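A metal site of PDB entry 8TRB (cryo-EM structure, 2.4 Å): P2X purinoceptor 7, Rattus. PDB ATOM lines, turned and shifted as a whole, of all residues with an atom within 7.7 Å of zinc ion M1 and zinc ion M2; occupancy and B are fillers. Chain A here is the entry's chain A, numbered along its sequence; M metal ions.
Zinc ion M2 is bound by SG of Cys 572 (2.3 Å). Zinc ion M2 is bound by SG of Cys 506 (2.3 Å). Zinc ion M2 is bound by SG of Cys 499 (2.3 Å). The side-chain sulfur (SG) of Cys 479 is bound to zinc ion M2, at 2.3 Å. Zinc ion M2 has four donor atoms within binding distance.
Zinc ion M1 is bound by SG of Cys 479, SG of Cys 482, SG of Cys 498 and SG of Cys 477. Zinc ion M1 has four donor atoms within binding distance.
The nearest printed residue that does not touch zinc ion M2 is Ile 507 (4.3 Å).
Merely in contact with zinc ion M1: Gln 478. Within 4 Å of zinc ion M1: Cys 477, Gln 478, Cys 479, Cys 482 and Cys 498.
The backbone NH (N) of Cys 572 sits close to the side-chain sulfur (SG) of Cys 482, 3.7 Å away. The side-chain sulfur (SG) of Cys 498 lies close to the backbone NH (N) of Gln 478, at 3.0 Å. The side-chain sulfur of Cys 498 sits close to the backbone carbonyl oxygen of Arg 500, 3.7 Å away. N of Cys 498 is in hydrogen-bond range of OE1 of Gln 422 (2.4 Å). The side-chain sulfur of Cys 477 lies close to the backbone NH of Gly 480, at 3.3 Å. The side-chain sulfur (SG) of Cys 506 lies close to the side-chain hydroxyl (OG1) of Thr 508 (2.8 Å). NE2 of Gln 478 lies within hydrogen-bond range of O of Trp 476, 3.5 Å away. O of Gln 478 sits at hydrogen-bond distance from N of Gly 504 (3.2 Å).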
ATOM      1  N   VAL A 404     -28.162  10.932  17.084  1.00  0.00           N
ATOM      2  CA  VAL A 404     -28.180   9.883  18.097  1.00  0.00           C
ATOM      3  C   VAL A 404     -29.108  10.264  19.237  1.00  0.00           C
ATOM      4  O   VAL A 404     -29.806   9.413  19.812  1.00  0.00           O
ATOM      5  CB  VAL A 404     -26.751   9.589  18.584  1.00  0.00           C
ATOM      6  CG1 VAL A 404     -26.224  10.741  19.398  1.00  0.00           C
ATOM      7  CG2 VAL A 404     -26.711   8.297  19.365  1.00  0.00           C
ATOM      8  N   GLN A 422     -26.808  21.020   9.414  1.00  0.00           N
ATOM      9  CA  GLN A 422     -27.285  20.853  10.787  1.00  0.00           C
ATOM     10  C   GLN A 422     -28.486  21.740  11.073  1.00  0.00           C
ATOM     11  O   GLN A 422     -29.327  21.384  11.910  1.00  0.00           O
ATOM     12  CB  GLN A 422     -26.145  21.163  11.753  1.00  0.00           C
ATOM     13  CG  GLN A 422     -26.467  20.898  13.208  1.00  0.00           C
ATOM     14  CD  GLN A 422     -26.089  19.504  13.648  1.00  0.00           C
ATOM     15  OE1 GLN A 422     -25.529  18.718  12.872  1.00  0.00           O
ATOM     16  NE2 GLN A 422     -26.402  19.179  14.880  1.00  0.00           N
ATOM     17  N   SER A 473     -14.046  24.161  18.775  1.00  0.00           N
ATOM     18  CA  SER A 473     -14.929  23.272  18.054  1.00  0.00           C
ATOM     19  C   SER A 473     -15.879  24.073  17.174  1.00  0.00           C
ATOM     20  O   SER A 473     -16.173  25.233  17.454  1.00  0.00           O
ATOM     21  CB  SER A 473     -15.728  22.407  19.039  1.00  0.00           C
ATOM     22  OG  SER A 473     -14.881  21.796  19.988  1.00  0.00           O
ATOM     23  N   PRO A 474     -16.374  23.473  16.089  1.00  0.00           N
ATOM     24  CA  PRO A 474     -17.301  24.198  15.220  1.00  0.00           C
ATOM     25  C   PRO A 474     -18.558  24.629  15.962  1.00  0.00           C
ATOM     26  O   PRO A 474     -19.012  23.962  16.890  1.00  0.00           O
ATOM     27  CB  PRO A 474     -17.625  23.174  14.120  1.00  0.00           C
ATOM     28  CG  PRO A 474     -16.501  22.224  14.141  1.00  0.00           C
ATOM     29  CD  PRO A 474     -16.055  22.139  15.559  1.00  0.00           C
ATOM     30  N   TRP A 476     -21.670  24.796  14.882  1.00  0.00           N
ATOM     31  CA  TRP A 476     -22.780  23.873  14.666  1.00  0.00           C
ATOM     32  C   TRP A 476     -22.560  22.519  15.335  1.00  0.00           C
ATOM     33  O   TRP A 476     -23.510  21.747  15.453  1.00  0.00           O
ATOM     34  CB  TRP A 476     -23.013  23.662  13.167  1.00  0.00           C
ATOM     35  CG  TRP A 476     -21.771  23.433  12.359  1.00  0.00           C
ATOM     36  CD1 TRP A 476     -21.115  24.344  11.602  1.00  0.00           C
ATOM     37  CD2 TRP A 476     -21.055  22.207  12.238  1.00  0.00           C
ATOM     38  NE1 TRP A 476     -20.022  23.775  11.002  1.00  0.00           N
ATOM     39  CE2 TRP A 476     -19.962  22.451  11.382  1.00  0.00           C
ATOM     40  CE3 TRP A 476     -21.218  20.921  12.764  1.00  0.00           C
ATOM     41  CZ2 TRP A 476     -19.037  21.471  11.043  1.00  0.00           C
ATOM     42  CZ3 TRP A 476     -20.304  19.953  12.427  1.00  0.00           C
ATOM     43  CH2 TRP A 476     -19.227  20.220  11.583  1.00  0.00           C
ATOM     44  N   CYS A 477     -21.338  22.219  15.774  1.00  0.00           N
ATOM     45  CA  CYS A 477     -21.072  20.959  16.429  1.00  0.00           C
ATOM     46  C   CYS A 477     -21.624  20.958  17.857  1.00  0.00           C
ATOM     47  O   CYS A 477     -21.800  22.011  18.476  1.00  0.00           O
ATOM     48  CB  CYS A 477     -19.585  20.659  16.454  1.00  0.00           C
ATOM     49  SG  CYS A 477     -19.132  19.265  17.500  1.00  0.00           S
ATOM     50  N   GLN A 478     -21.881  19.763  18.370  1.00  0.00           N
ATOM     51  CA  GLN A 478     -22.390  19.604  19.719  1.00  0.00           C
ATOM     52  C   GLN A 478     -21.737  18.414  20.422  1.00  0.00           C
ATOM     53  O   GLN A 478     -22.312  17.883  21.389  1.00  0.00           O
ATOM     54  CB  GLN A 478     -23.907  19.416  19.741  1.00  0.00           C
ATOM     55  CG  GLN A 478     -24.679  20.221  18.704  1.00  0.00           C
ATOM     56  CD  GLN A 478     -24.988  21.629  19.160  1.00  0.00           C
ATOM     57  OE1 GLN A 478     -24.808  21.972  20.327  1.00  0.00           O
ATOM     58  NE2 GLN A 478     -25.439  22.453  18.227  1.00  0.00           N
ATOM     59  N   CYS A 479     -20.584  17.958  19.952  1.00  0.00           N
ATOM     60  CA  CYS A 479     -19.930  16.795  20.543  1.00  0.00           C
ATOM     61  C   CYS A 479     -18.431  16.944  20.722  1.00  0.00           C
ATOM     62  O   CYS A 479     -17.821  16.074  21.353  1.00  0.00           O
ATOM     63  CB  CYS A 479     -20.212  15.542  19.704  1.00  0.00           C
ATOM     64  SG  CYS A 479     -19.474  15.529  18.052  1.00  0.00           S
ATOM     65  N   GLY A 480     -17.800  18.000  20.204  1.00  0.00           N
ATOM     66  CA  GLY A 480     -16.401  18.229  20.427  1.00  0.00           C
ATOM     67  C   GLY A 480     -15.460  17.431  19.542  1.00  0.00           C
ATOM     68  O   GLY A 480     -14.254  17.432  19.795  1.00  0.00           O
ATOM     69  N   ASN A 481     -15.981  16.751  18.518  1.00  0.00           N
ATOM     70  CA  ASN A 481     -15.168  15.951  17.617  1.00  0.00           C
ATOM     71  C   ASN A 481     -15.310  16.343  16.166  1.00  0.00           C
ATOM     72  O   ASN A 481     -14.470  15.941  15.347  1.00  0.00           O
ATOM     73  CB  ASN A 481     -15.518  14.460  17.757  1.00  0.00           C
ATOM     74  CG  ASN A 481     -15.485  13.979  19.188  1.00  0.00           C
ATOM     75  OD1 ASN A 481     -16.252  14.436  20.029  1.00  0.00           O
ATOM     76  ND2 ASN A 481     -14.588  13.050  19.475  1.00  0.00           N
ATOM     77  N   CYS A 482     -16.323  17.116  15.810  1.00  0.00           N
ATOM     78  CA  CYS A 482     -16.513  17.534  14.433  1.00  0.00           C
ATOM     79  C   CYS A 482     -15.430  18.531  14.021  1.00  0.00           C
ATOM     80  O   CYS A 482     -15.052  19.409  14.790  1.00  0.00           O
ATOM     81  CB  CYS A 482     -17.890  18.158  14.249  1.00  0.00           C
ATOM     82  SG  CYS A 482     -19.263  17.015  14.506  1.00  0.00           S
ATOM     83  N   LEU A 483     -14.939  18.379  12.797  1.00  0.00           N
ATOM     84  CA  LEU A 483     -13.919  19.243  12.252  1.00  0.00           C
ATOM     85  C   LEU A 483     -14.467  20.021  11.057  1.00  0.00           C
ATOM     86  O   LEU A 483     -15.397  19.558  10.389  1.00  0.00           O
ATOM     87  CB  LEU A 483     -12.680  18.460  11.811  1.00  0.00           C
ATOM     88  CG  LEU A 483     -12.336  17.178  12.561  1.00  0.00           C
ATOM     89  CD1 LEU A 483     -11.094  16.547  11.961  1.00  0.00           C
ATOM     90  CD2 LEU A 483     -12.141  17.450  14.028  1.00  0.00           C
ATOM     91  N   LEU A 497     -22.334  18.859   9.522  1.00  0.00           N
ATOM     92  CA  LEU A 497     -23.331  18.102  10.245  1.00  0.00           C
ATOM     93  C   LEU A 497     -22.709  17.450  11.469  1.00  0.00           C
ATOM     94  O   LEU A 497     -21.605  16.888  11.392  1.00  0.00           O
ATOM     95  CB  LEU A 497     -23.959  17.038   9.339  1.00  0.00           C
ATOM     96  CG  LEU A 497     -25.082  16.191   9.944  1.00  0.00           C
ATOM     97  CD1 LEU A 497     -26.369  16.964  10.032  1.00  0.00           C
ATOM     98  CD2 LEU A 497     -25.245  14.934   9.115  1.00  0.00           C
ATOM     99  N   CYS A 498     -23.415  17.530  12.583  1.00  0.00           N
ATOM    100  CA  CYS A 498     -22.997  16.929  13.843  1.00  0.00           C
ATOM    101  C   CYS A 498     -23.789  15.656  14.093  1.00  0.00           C
ATOM    102  O   CYS A 498     -24.915  15.489  13.604  1.00  0.00           O
ATOM    103  CB  CYS A 498     -23.197  17.904  15.004  1.00  0.00           C
ATOM    104  SG  CYS A 498     -22.374  17.447  16.539  1.00  0.00           S
ATOM    105  N   CYS A 499     -23.191  14.740  14.844  1.00  0.00           N
ATOM    106  CA  CYS A 499     -23.839  13.483  15.195  1.00  0.00           C
ATOM    107  C   CYS A 499     -25.062  13.675  16.068  1.00  0.00           C
ATOM    108  O   CYS A 499     -25.856  12.727  16.190  1.00  0.00           O
ATOM    109  CB  CYS A 499     -22.833  12.568  15.891  1.00  0.00           C
ATOM    110  SG  CYS A 499     -22.290  13.137  17.505  1.00  0.00           S
ATOM    111  N   ARG A 500     -25.247  14.843  16.670  1.00  0.00           N
ATOM    112  CA  ARG A 500     -26.379  15.077  17.555  1.00  0.00           C
ATOM    113  C   ARG A 500     -26.804  16.531  17.458  1.00  0.00           C
ATOM    114  O   ARG A 500     -26.003  17.409  17.114  1.00  0.00           O
ATOM    115  CB  ARG A 500     -26.033  14.725  18.999  1.00  0.00           C
ATOM    116  CG  ARG A 500     -24.763  15.383  19.511  1.00  0.00           C
ATOM    117  CD  ARG A 500     -24.370  14.862  20.869  1.00  0.00           C
ATOM    118  NE  ARG A 500     -25.538  14.565  21.689  1.00  0.00           N
ATOM    119  CZ  ARG A 500     -25.672  13.483  22.451  1.00  0.00           C
ATOM    120  NH1 ARG A 500     -24.715  12.564  22.522  1.00  0.00           N
ATOM    121  NH2 ARG A 500     -26.783  13.314  23.152  1.00  0.00           N
ATOM    122  N   GLY A 504     -23.669  16.648  24.013  1.00  0.00           N
ATOM    123  CA  GLY A 504     -23.634  15.336  24.620  1.00  0.00           C
ATOM    124  C   GLY A 504     -22.418  14.559  24.162  1.00  0.00           C
ATOM    125  O   GLY A 504     -21.528  15.099  23.492  1.00  0.00           O
ATOM    126  N   GLN A 505     -22.394  13.283  24.537  1.00  0.00           N
ATOM    127  CA  GLN A 505     -21.296  12.414  24.138  1.00  0.00           C
ATOM    128  C   GLN A 505     -21.398  12.073  22.658  1.00  0.00           C
ATOM    129  O   GLN A 505     -22.488  11.861  22.123  1.00  0.00           O
ATOM    130  CB  GLN A 505     -21.300  11.137  24.985  1.00  0.00           C
ATOM    131  CG  GLN A 505     -22.586  10.344  24.916  1.00  0.00           C
ATOM    132  CD  GLN A 505     -22.524   9.066  25.724  1.00  0.00           C
ATOM    133  OE1 GLN A 505     -21.466   8.440  25.842  1.00  0.00           O
ATOM    134  NE2 GLN A 505     -23.663   8.665  26.279  1.00  0.00           N
ATOM    135  N   CYS A 506     -20.249  12.017  22.002  1.00  0.00           N
ATOM    136  CA  CYS A 506     -20.221  11.686  20.589  1.00  0.00           C
ATOM    137  C   CYS A 506     -20.556  10.214  20.369  1.00  0.00           C
ATOM    138  O   CYS A 506     -20.242   9.343  21.197  1.00  0.00           O
ATOM    139  CB  CYS A 506     -18.840  11.978  19.994  1.00  0.00           C
ATOM    140  SG  CYS A 506     -18.772  11.804  18.201  1.00  0.00           S
ATOM    141  N   ILE A 507     -21.206   9.935  19.244  1.00  0.00           N
ATOM    142  CA  ILE A 507     -21.503   8.566  18.870  1.00  0.00           C
ATOM    143  C   ILE A 507     -20.230   7.774  18.638  1.00  0.00           C
ATOM    144  O   ILE A 507     -20.204   6.552  18.789  1.00  0.00           O
ATOM    145  CB  ILE A 507     -22.408   8.552  17.614  1.00  0.00           C
ATOM    146  CG1 ILE A 507     -23.071   7.185  17.448  1.00  0.00           C
ATOM    147  CG2 ILE A 507     -21.600   8.897  16.387  1.00  0.00           C
ATOM    148  CD1 ILE A 507     -24.050   7.138  16.315  1.00  0.00           C
ATOM    149  N   THR A 508     -19.144   8.461  18.254  1.00  0.00           N
ATOM    150  CA  THR A 508     -17.881   7.773  18.019  1.00  0.00           C
ATOM    151  C   THR A 508     -17.370   7.081  19.278  1.00  0.00           C
ATOM    152  O   THR A 508     -16.650   6.079  19.177  1.00  0.00           O
ATOM    153  CB  THR A 508     -16.830   8.762  17.510  1.00  0.00           C
ATOM    154  OG1 THR A 508     -16.779   9.897  18.382  1.00  0.00           O
ATOM    155  CG2 THR A 508     -17.169   9.223  16.110  1.00  0.00           C
ATOM    156  N   THR A 509     -17.718   7.595  20.449  1.00  0.00           N
ATOM    157  CA  THR A 509     -17.256   7.006  21.689  1.00  0.00           C
ATOM    158  C   THR A 509     -17.950   5.689  22.013  1.00  0.00           C
ATOM    159  O   THR A 509     -17.490   4.958  22.896  1.00  0.00           O
ATOM    160  CB  THR A 509     -17.455   7.991  22.851  1.00  0.00           C
ATOM    161  OG1 THR A 509     -18.859   8.208  23.065  1.00  0.00           O
ATOM    162  CG2 THR A 509     -16.787   9.324  22.533  1.00  0.00           C
ATOM    163  N   TYR A 553     -21.698   2.556   8.612  1.00  0.00           N
ATOM    164  CA  TYR A 553     -22.352   3.542   9.463  1.00  0.00           C
ATOM    165  C   TYR A 553     -23.732   3.900   8.931  1.00  0.00           C
ATOM    166  O   TYR A 553     -24.700   4.005   9.686  1.00  0.00           O
ATOM    167  CB  TYR A 553     -21.498   4.799   9.590  1.00  0.00           C
ATOM    168  CG  TYR A 553     -22.161   5.881  10.401  1.00  0.00           C
ATOM    169  CD1 TYR A 553     -23.021   6.791   9.797  1.00  0.00           C
ATOM    170  CD2 TYR A 553     -21.949   6.002  11.759  1.00  0.00           C
ATOM    171  CE1 TYR A 553     -23.637   7.775  10.528  1.00  0.00           C
ATOM    172  CE2 TYR A 553     -22.559   6.974  12.494  1.00  0.00           C
ATOM    173  CZ  TYR A 553     -23.403   7.861  11.879  1.00  0.00           C
ATOM    174  OH  TYR A 553     -24.019   8.857  12.596  1.00  0.00           O
ATOM    175  N   PRO A 570     -21.998  12.288   9.783  1.00  0.00           N
ATOM    176  CA  PRO A 570     -21.534  13.444  10.564  1.00  0.00           C
ATOM    177  C   PRO A 570     -20.047  13.680  10.357  1.00  0.00           C
ATOM    178  O   PRO A 570     -19.292  12.767  10.015  1.00  0.00           O
ATOM    179  CB  PRO A 570     -21.849  13.046  11.998  1.00  0.00           C
ATOM    180  CG  PRO A 570     -22.806  11.940  11.908  1.00  0.00           C
ATOM    181  CD  PRO A 570     -22.511  11.227  10.655  1.00  0.00           C
ATOM    182  N   SER A 571     -19.646  14.924  10.582  1.00  0.00           N
ATOM    183  CA  SER A 571     -18.248  15.279  10.400  1.00  0.00           C
ATOM    184  C   SER A 571     -17.344  14.483  11.345  1.00  0.00           C
ATOM    185  O   SER A 571     -16.253  14.055  10.952  1.00  0.00           O
ATOM    186  CB  SER A 571     -18.046  16.779  10.621  1.00  0.00           C
ATOM    187  OG  SER A 571     -18.731  17.532   9.638  1.00  0.00           O
ATOM    188  N   CYS A 572     -17.794  14.278  12.580  1.00  0.00           N
ATOM    189  CA  CYS A 572     -16.961  13.577  13.552  1.00  0.00           C
ATOM    190  C   CYS A 572     -16.691  12.146  13.107  1.00  0.00           C
ATOM    191  O   CYS A 572     -15.539  11.707  13.041  1.00  0.00           O
ATOM    192  CB  CYS A 572     -17.630  13.593  14.920  1.00  0.00           C
ATOM    193  SG  CYS A 572     -19.434  13.489  14.879  1.00  0.00           S
ATOM    194  N   CYS A 573     -17.755  11.404  12.786  1.00  0.00           N
ATOM    195  CA  CYS A 573     -17.600  10.028  12.328  1.00  0.00           C
ATOM    196  C   CYS A 573     -16.845   9.971  11.000  1.00  0.00           C
ATOM    197  O   CYS A 573     -15.980   9.118  10.804  1.00  0.00           O
ATOM    198  CB  CYS A 573     -18.969   9.377  12.213  1.00  0.00           C
ATOM    199  SG  CYS A 573     -20.053   9.755  13.599  1.00  0.00           S
HETATM  200 ZN    ZN M   1     -20.057  17.297  16.672  1.00  0.00          ZN
HETATM  201 ZN    ZN M   2     -20.012  13.455  17.127  1.00  0.00          ZN
